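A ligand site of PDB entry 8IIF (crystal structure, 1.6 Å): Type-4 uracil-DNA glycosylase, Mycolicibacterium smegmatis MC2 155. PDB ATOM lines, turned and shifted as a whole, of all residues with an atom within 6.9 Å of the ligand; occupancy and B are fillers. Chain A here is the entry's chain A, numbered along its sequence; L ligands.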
ATOM      1  N   GLY A   2     -10.377 -19.999  23.107  1.00  0.00           N
ATOM      2  CA  GLY A   2      -9.364 -19.105  23.656  1.00  0.00           C
ATOM      3  C   GLY A   2      -9.012 -19.416  25.106  1.00  0.00           C
ATOM      4  O   GLY A   2      -8.811 -20.565  25.503  1.00  0.00           O
ATOM      5  N   ALA A   3      -8.900 -18.347  25.904  1.00  0.00           N
ATOM      6  CA  ALA A   3      -8.536 -18.447  27.305  1.00  0.00           C
ATOM      7  C   ALA A   3      -9.676 -18.866  28.216  1.00  0.00           C
ATOM      8  O   ALA A   3      -9.437 -19.058  29.407  1.00  0.00           O
ATOM      9  CB  ALA A   3      -8.004 -17.097  27.799  1.00  0.00           C
ATOM     10  N   PHE A   6      -9.467 -21.343  31.084  1.00  0.00           N
ATOM     11  CA  PHE A   6      -8.388 -21.084  32.030  1.00  0.00           C
ATOM     12  C   PHE A   6      -8.766 -20.051  33.084  1.00  0.00           C
ATOM     13  O   PHE A   6      -8.049 -19.918  34.071  1.00  0.00           O
ATOM     14  CB  PHE A   6      -7.135 -20.624  31.278  1.00  0.00           C
ATOM     15  CG  PHE A   6      -6.560 -21.690  30.383  1.00  0.00           C
ATOM     16  CD1 PHE A   6      -5.787 -22.713  30.902  1.00  0.00           C
ATOM     17  CD2 PHE A   6      -6.825 -21.684  29.012  1.00  0.00           C
ATOM     18  CE1 PHE A   6      -5.257 -23.701  30.058  1.00  0.00           C
ATOM     19  CE2 PHE A   6      -6.311 -22.670  28.176  1.00  0.00           C
ATOM     20  CZ  PHE A   6      -5.521 -23.670  28.707  1.00  0.00           C
ATOM     21  N   ALA A  20      -3.810 -16.830  35.316  1.00  0.00           N
ATOM     22  CA  ALA A  20      -3.300 -16.410  34.013  1.00  0.00           C
ATOM     23  C   ALA A  20      -1.881 -16.910  33.790  1.00  0.00           C
ATOM     24  O   ALA A  20      -1.477 -17.122  32.638  1.00  0.00           O
ATOM     25  CB  ALA A  20      -3.356 -14.890  33.878  1.00  0.00           C
ATOM     26  N   GLY A  21      -1.128 -17.106  34.868  1.00  0.00           N
ATOM     27  CA  GLY A  21       0.195 -17.700  34.736  1.00  0.00           C
ATOM     28  C   GLY A  21       0.152 -19.096  34.167  1.00  0.00           C
ATOM     29  O   GLY A  21       1.158 -19.570  33.625  1.00  0.00           O
ATOM     30  N   GLU A  22      -1.009 -19.729  34.203  1.00  0.00           N
ATOM     31  CA  GLU A  22      -1.137 -21.122  33.694  1.00  0.00           C
ATOM     32  C   GLU A  22      -1.901 -21.127  32.364  1.00  0.00           C
ATOM     33  O   GLU A  22      -2.168 -22.197  31.854  1.00  0.00           O
ATOM     34  CB  GLU A  22      -1.880 -22.037  34.676  1.00  0.00           C
ATOM     35  CG  GLU A  22      -1.450 -21.870  36.119  1.00  0.00           C
ATOM     36  CD  GLU A  22      -0.121 -22.518  36.470  1.00  0.00           C
ATOM     37  OE1 GLU A  22       0.489 -23.135  35.583  1.00  0.00           O
ATOM     38  OE2 GLU A  22       0.290 -22.412  37.633  1.00  0.00           O
ATOM     39  N   CYS A  23      -2.218 -19.949  31.832  1.00  0.00           N
ATOM     40  CA  CYS A  23      -3.038 -19.913  30.613  1.00  0.00           C
ATOM     41  C   CYS A  23      -2.257 -20.395  29.406  1.00  0.00           C
ATOM     42  O   CYS A  23      -1.089 -20.052  29.219  1.00  0.00           O
ATOM     43  CB  CYS A  23      -3.542 -18.488  30.374  1.00  0.00           C
ATOM     44  SG  CYS A  23      -4.690 -18.339  28.970  1.00  0.00           S
ATOM     45  N   ARG A  24      -2.926 -21.199  28.556  1.00  0.00           N
ATOM     46  CA  ARG A  24      -2.416 -21.630  27.265  1.00  0.00           C
ATOM     47  C   ARG A  24      -3.406 -21.273  26.165  1.00  0.00           C
ATOM     48  O   ARG A  24      -3.468 -21.939  25.138  1.00  0.00           O
ATOM     49  CB  ARG A  24      -2.124 -23.128  27.268  1.00  0.00           C
ATOM     50  CG  ARG A  24      -1.128 -23.538  28.356  1.00  0.00           C
ATOM     51  CD  ARG A  24      -0.657 -24.993  28.192  1.00  0.00           C
ATOM     52  NE  ARG A  24      -1.795 -25.861  27.917  1.00  0.00           N
ATOM     53  CZ  ARG A  24      -2.606 -26.335  28.861  1.00  0.00           C
ATOM     54  NH1 ARG A  24      -2.420 -26.034  30.139  1.00  0.00           N
ATOM     55  NH2 ARG A  24      -3.644 -27.090  28.506  1.00  0.00           N
ATOM     56  N   GLY A  25      -4.187 -20.204  26.389  1.00  0.00           N
ATOM     57  CA  GLY A  25      -5.331 -19.859  25.537  1.00  0.00           C
ATOM     58  C   GLY A  25      -4.958 -19.469  24.114  1.00  0.00           C
ATOM     59  O   GLY A  25      -5.820 -19.530  23.230  1.00  0.00           O
ATOM     60  N   CYS A  26      -3.715 -19.054  23.886  1.00  0.00           N
ATOM     61  CA  CYS A  26      -3.186 -18.868  22.542  1.00  0.00           C
ATOM     62  C   CYS A  26      -1.721 -19.294  22.582  1.00  0.00           C
ATOM     63  O   CYS A  26      -1.272 -19.906  23.543  1.00  0.00           O
ATOM     64  CB  CYS A  26      -3.391 -17.424  22.058  1.00  0.00           C
ATOM     65  SG  CYS A  26      -2.298 -16.170  22.818  1.00  0.00           S
ATOM     66  N   GLY A  27      -0.974 -18.998  21.521  1.00  0.00           N
ATOM     67  CA  GLY A  27       0.400 -19.477  21.525  1.00  0.00           C
ATOM     68  C   GLY A  27       1.383 -18.631  22.300  1.00  0.00           C
ATOM     69  O   GLY A  27       2.540 -19.032  22.466  1.00  0.00           O
ATOM     70  N   LEU A  28       0.968 -17.463  22.786  1.00  0.00           N
ATOM     71  CA  LEU A  28       1.953 -16.477  23.228  1.00  0.00           C
ATOM     72  C   LEU A  28       2.614 -16.849  24.541  1.00  0.00           C
ATOM     73  O   LEU A  28       3.696 -16.309  24.844  1.00  0.00           O
ATOM     74  CB  LEU A  28       1.314 -15.088  23.330  1.00  0.00           C
ATOM     75  CG  LEU A  28       0.842 -14.544  21.982  1.00  0.00           C
ATOM     76  CD1 LEU A  28       0.233 -13.147  22.157  1.00  0.00           C
ATOM     77  CD2 LEU A  28       2.025 -14.490  21.003  1.00  0.00           C
ATOM     78  N   TYR A  29       2.022 -17.763  25.320  1.00  0.00           N
ATOM     79  CA  TYR A  29       2.633 -18.148  26.598  1.00  0.00           C
ATOM     80  C   TYR A  29       3.972 -18.845  26.407  1.00  0.00           C
ATOM     81  O   TYR A  29       4.780 -18.881  27.340  1.00  0.00           O
ATOM     82  CB  TYR A  29       1.683 -19.056  27.388  1.00  0.00           C
ATOM     83  CG  TYR A  29       1.654 -20.472  26.846  1.00  0.00           C
ATOM     84  CD1 TYR A  29       0.796 -20.813  25.803  1.00  0.00           C
ATOM     85  CD2 TYR A  29       2.491 -21.461  27.362  1.00  0.00           C
ATOM     86  CE1 TYR A  29       0.765 -22.098  25.292  1.00  0.00           C
ATOM     87  CE2 TYR A  29       2.469 -22.756  26.847  1.00  0.00           C
ATOM     88  CZ  TYR A  29       1.604 -23.063  25.828  1.00  0.00           C
ATOM     89  OH  TYR A  29       1.561 -24.333  25.305  1.00  0.00           O
ATOM     90  N   ARG A  30       4.167 -19.402  25.212  1.00  0.00           N
ATOM     91  CA  ARG A  30       5.370 -20.252  25.037  1.00  0.00           C
ATOM     92  C   ARG A  30       6.672 -19.457  25.139  1.00  0.00           C
ATOM     93  O   ARG A  30       7.542 -19.895  25.872  1.00  0.00           O
ATOM     94  CB  ARG A  30       5.332 -21.064  23.733  1.00  0.00           C
ATOM     95  CG  ARG A  30       4.279 -22.147  23.684  1.00  0.00           C
ATOM     96  CD  ARG A  30       4.457 -23.047  22.471  1.00  0.00           C
ATOM     97  N   ALA A  35       3.151 -14.497  32.327  1.00  0.00           N
ATOM     98  CA  ALA A  35       1.990 -13.652  32.092  1.00  0.00           C
ATOM     99  C   ALA A  35       2.163 -12.359  32.875  1.00  0.00           C
ATOM    100  O   ALA A  35       2.746 -12.342  33.963  1.00  0.00           O
ATOM    101  CB  ALA A  35       0.697 -14.357  32.531  1.00  0.00           C
ATOM    102  N   ALA A  91      -4.487  -5.694  26.605  1.00  0.00           N
ATOM    103  CA  ALA A  91      -5.433  -6.536  25.881  1.00  0.00           C
ATOM    104  C   ALA A  91      -4.949  -7.969  25.814  1.00  0.00           C
ATOM    105  O   ALA A  91      -5.746  -8.911  25.896  1.00  0.00           O
ATOM    106  CB  ALA A  91      -5.632  -5.985  24.465  1.00  0.00           C
ATOM    107  N   VAL A  92      -3.642  -8.175  25.665  1.00  0.00           N
ATOM    108  CA  VAL A  92      -3.099  -9.520  25.766  1.00  0.00           C
ATOM    109  C   VAL A  92      -2.059  -9.550  26.873  1.00  0.00           C
ATOM    110  O   VAL A  92      -1.431  -8.528  27.194  1.00  0.00           O
ATOM    111  CB  VAL A  92      -2.531 -10.074  24.433  1.00  0.00           C
ATOM    112  CG1 VAL A  92      -3.576  -9.975  23.300  1.00  0.00           C
ATOM    113  CG2 VAL A  92      -1.266  -9.393  24.056  1.00  0.00           C
ATOM    114  N   LYS A  93      -1.902 -10.713  27.509  1.00  0.00           N
ATOM    115  CA  LYS A  93      -1.112 -10.822  28.775  1.00  0.00           C
ATOM    116  C   LYS A  93       0.274 -11.465  28.638  1.00  0.00           C
ATOM    117  O   LYS A  93       0.978 -11.514  29.605  1.00  0.00           O
ATOM    118  CB  LYS A  93      -1.917 -11.698  29.746  1.00  0.00           C
ATOM    119  CG  LYS A  93      -2.802 -11.006  30.766  1.00  0.00           C
ATOM    120  CD  LYS A  93      -3.739 -10.012  30.184  1.00  0.00           C
ATOM    121  CE  LYS A  93      -4.710  -9.472  31.214  1.00  0.00           C
ATOM    122  NZ  LYS A  93      -5.697  -8.580  30.562  1.00  0.00           N
ATOM    123  N   HIS A  94       0.615 -11.932  27.448  1.00  0.00           N
ATOM    124  CA  HIS A  94       1.976 -12.464  27.192  1.00  0.00           C
ATOM    125  C   HIS A  94       2.643 -11.652  26.064  1.00  0.00           C
ATOM    126  O   HIS A  94       1.965 -11.324  25.088  1.00  0.00           O
ATOM    127  CB  HIS A  94       1.989 -13.951  26.879  1.00  0.00           C
ATOM    128  CG  HIS A  94       1.845 -14.863  28.062  1.00  0.00           C
ATOM    129  ND1 HIS A  94       0.637 -15.477  28.300  1.00  0.00           N
ATOM    130  CD2 HIS A  94       2.722 -15.327  28.988  1.00  0.00           C
ATOM    131  CE1 HIS A  94       0.744 -16.251  29.356  1.00  0.00           C
ATOM    132  NE2 HIS A  94       2.000 -16.185  29.771  1.00  0.00           N
ATOM    133  N   PHE A  95       3.911 -11.353  26.242  1.00  0.00           N
ATOM    134  CA  PHE A  95       4.642 -10.531  25.274  1.00  0.00           C
ATOM    135  C   PHE A  95       4.867 -11.313  23.972  1.00  0.00           C
ATOM    136  O   PHE A  95       5.323 -12.430  24.048  1.00  0.00           O
ATOM    137  CB  PHE A  95       5.980 -10.169  25.910  1.00  0.00           C
ATOM    138  CG  PHE A  95       6.949  -9.303  25.141  1.00  0.00           C
ATOM    139  CD1 PHE A  95       6.516  -8.293  24.306  1.00  0.00           C
ATOM    140  CD2 PHE A  95       8.304  -9.470  25.315  1.00  0.00           C
ATOM    141  CE1 PHE A  95       7.423  -7.484  23.643  1.00  0.00           C
ATOM    142  CE2 PHE A  95       9.212  -8.667  24.644  1.00  0.00           C
ATOM    143  CZ  PHE A  95       8.769  -7.677  23.810  1.00  0.00           C
ATOM    144  N   GLU A 115      -5.483 -13.635  18.603  1.00  0.00           N
ATOM    145  CA  GLU A 115      -4.896 -13.615  19.973  1.00  0.00           C
ATOM    146  C   GLU A 115      -5.680 -12.672  20.890  1.00  0.00           C
ATOM    147  O   GLU A 115      -5.898 -13.002  22.032  1.00  0.00           O
ATOM    148  CB  GLU A 115      -3.427 -13.166  19.911  1.00  0.00           C
ATOM    149  CG  GLU A 115      -2.537 -14.288  19.393  1.00  0.00           C
ATOM    150  CD  GLU A 115      -1.280 -13.904  18.634  1.00  0.00           C
ATOM    151  OE1 GLU A 115      -1.097 -12.718  18.373  1.00  0.00           O
ATOM    152  OE2 GLU A 115      -0.501 -14.801  18.325  1.00  0.00           O
ATOM    153  N   VAL A 116      -6.057 -11.515  20.365  1.00  0.00           N
ATOM    154  CA  VAL A 116      -6.793 -10.542  21.230  1.00  0.00           C
ATOM    155  C   VAL A 116      -8.105 -11.198  21.682  1.00  0.00           C
ATOM    156  O   VAL A 116      -8.463 -11.105  22.851  1.00  0.00           O
ATOM    157  CB  VAL A 116      -7.072  -9.232  20.462  1.00  0.00           C
ATOM    158  CG1 VAL A 116      -8.048  -8.321  21.166  1.00  0.00           C
ATOM    159  CG2 VAL A 116      -5.796  -8.501  20.112  1.00  0.00           C
ATOM    160  N   VAL A 117      -8.793 -11.824  20.740  1.00  0.00           N
ATOM    161  CA  VAL A 117     -10.106 -12.439  21.076  1.00  0.00           C
ATOM    162  C   VAL A 117      -9.879 -13.624  22.033  1.00  0.00           C
ATOM    163  O   VAL A 117     -10.677 -13.804  22.929  1.00  0.00           O
ATOM    164  CB  VAL A 117     -10.925 -12.826  19.824  1.00  0.00           C
ATOM    165  CG1 VAL A 117     -12.137 -13.672  20.153  1.00  0.00           C
ATOM    166  CG2 VAL A 117     -11.338 -11.597  19.034  1.00  0.00           C
ATOM    167  N   ALA A 118      -8.780 -14.352  21.843  1.00  0.00           N
ATOM    168  CA  ALA A 118      -8.479 -15.495  22.730  1.00  0.00           C
ATOM    169  C   ALA A 118      -8.285 -14.995  24.164  1.00  0.00           C
ATOM    170  O   ALA A 118      -8.694 -15.685  25.055  1.00  0.00           O
ATOM    171  CB  ALA A 118      -7.209 -16.195  22.272  1.00  0.00           C
ATOM    172  N   CYS A 119      -7.606 -13.855  24.309  1.00  0.00           N
ATOM    173  CA  CYS A 119      -7.242 -13.355  25.655  1.00  0.00           C
ATOM    174  C   CYS A 119      -8.363 -12.546  26.289  1.00  0.00           C
ATOM    175  O   CYS A 119      -8.296 -12.281  27.479  1.00  0.00           O
ATOM    176  CB  CYS A 119      -6.021 -12.451  25.521  1.00  0.00           C
ATOM    177  SG  CYS A 119      -4.988 -12.408  27.032  1.00  0.00           S
ATOM    178  N   ARG A 120      -9.277 -12.096  25.455  1.00  0.00           N
ATOM    179  CA  ARG A 120     -10.359 -11.207  25.951  1.00  0.00           C
ATOM    180  C   ARG A 120     -11.037 -11.746  27.218  1.00  0.00           C
ATOM    181  O   ARG A 120     -11.383 -10.915  28.025  1.00  0.00           O
ATOM    182  CB  ARG A 120     -11.342 -10.788  24.846  1.00  0.00           C
ATOM    183  CG  ARG A 120     -12.068  -9.485  25.158  1.00  0.00           C
ATOM    184  CD  ARG A 120     -12.812  -8.966  23.940  1.00  0.00           C
ATOM    185  NE  ARG A 120     -13.513 -10.003  23.214  1.00  0.00           N
ATOM    186  CZ  ARG A 120     -13.938  -9.863  21.961  1.00  0.00           C
ATOM    187  NH1 ARG A 120     -13.729  -8.734  21.324  1.00  0.00           N
ATOM    188  NH2 ARG A 120     -14.578 -10.855  21.359  1.00  0.00           N
ATOM    189  N   PRO A 121     -11.285 -13.061  27.414  1.00  0.00           N
ATOM    190  CA  PRO A 121     -11.875 -13.513  28.680  1.00  0.00           C
ATOM    191  C   PRO A 121     -11.196 -12.971  29.951  1.00  0.00           C
ATOM    192  O   PRO A 121     -11.829 -12.775  30.912  1.00  0.00           O
ATOM    193  CB  PRO A 121     -11.728 -15.030  28.591  1.00  0.00           C
ATOM    194  CG  PRO A 121     -11.906 -15.336  27.133  1.00  0.00           C
ATOM    195  CD  PRO A 121     -11.267 -14.154  26.441  1.00  0.00           C
ATOM    196  N   TRP A 122      -9.879 -12.762  29.904  1.00  0.00           N
ATOM    197  CA  TRP A 122      -9.170 -12.178  31.075  1.00  0.00           C
ATOM    198  C   TRP A 122      -9.611 -10.721  31.278  1.00  0.00           C
ATOM    199  O   TRP A 122      -9.839 -10.340  32.396  1.00  0.00           O
ATOM    200  CB  TRP A 122      -7.645 -12.269  30.922  1.00  0.00           C
ATOM    201  CG  TRP A 122      -7.132 -13.676  30.976  1.00  0.00           C
ATOM    202  CD1 TRP A 122      -6.537 -14.370  29.968  1.00  0.00           C
ATOM    203  CD2 TRP A 122      -7.178 -14.553  32.110  1.00  0.00           C
ATOM    204  NE1 TRP A 122      -6.220 -15.632  30.387  1.00  0.00           N
ATOM    205  CE2 TRP A 122      -6.594 -15.774  31.696  1.00  0.00           C
ATOM    206  CE3 TRP A 122      -7.652 -14.440  33.422  1.00  0.00           C
ATOM    207  CZ2 TRP A 122      -6.482 -16.863  32.557  1.00  0.00           C
ATOM    208  CZ3 TRP A 122      -7.529 -15.521  34.266  1.00  0.00           C
ATOM    209  CH2 TRP A 122      -6.960 -16.710  33.840  1.00  0.00           C
HETATM  210 FE1  LIG L   1      -3.696 -14.295  26.852  1.00  0.00          FE
HETATM  211 FE2  LIG L   1      -2.706 -16.068  25.071  1.00  0.00          FE
HETATM  212 FE3  LIG L   1      -3.551 -16.901  27.510  1.00  0.00          FE
HETATM  213 FE4  LIG L   1      -1.316 -15.490  27.274  1.00  0.00          FE
HETATM  214  S1  LIG L   1      -1.632 -17.592  26.442  1.00  0.00           S
HETATM  215  S2  LIG L   1      -2.950 -15.122  28.856  1.00  0.00           S
HETATM  216  S3  LIG L   1      -1.789 -14.003  25.590  1.00  0.00           S
HETATM  217  S4  LIG L   1      -4.841 -16.052  25.862  1.00  0.00           S
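Merely in contact with the ligand: Ala 3, Leu 28, Tyr 29, Lys 93 and Ala 118. Of the 28 residues printed, 11 come within 4 Å of the ligand. The nearest printed residue that does not touch the ligand is Arg 24 (4.1 Å).
N of Gly 25 lies close to S1 of the ligand. SG of Cys 26 is bound to FE2 of the ligand (2.3 Å). An iron atom (FE1) of the ligand is bound by the side-chain sulfur (SG) of Cys 119, 2.3 Å away. S2 of the ligand lies close to NE1 of Trp 122 (3.6 Å). S3 of the ligand lies close to N of His 94. An iron atom (FE4) of the ligand is bound by a ring nitrogen (ND1) of His 94, at 2.2 Å. SG of Cys 23 binds FE3 of the ligand, at 2.3 Å. N of Cys 26 lies close to S1 of the ligand, at 3.6 Å.
SG of Cys 26 sits close to N of Leu 28 (3.5 Å). The backbone NH (N) of Gly 25 sits close to the side-chain sulfur (SG) of Cys 23 (3.2 Å). The backbone NH of Ala 35 lies within hydrogen-bond range of a ring nitrogen (NE2) of His 94 (3.3 Å). SG of Cys 119 lies close to N of Lys 93, 3.6 Å away. SG of Cys 23 lies close to NE1 of Trp 122 (3.4 Å). N of Ala 3 lies within hydrogen-bond range of O of Ala 118, 2.8 Å away. SG of Cys 119 sits close to O of Ala 91 (3.8 Å).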
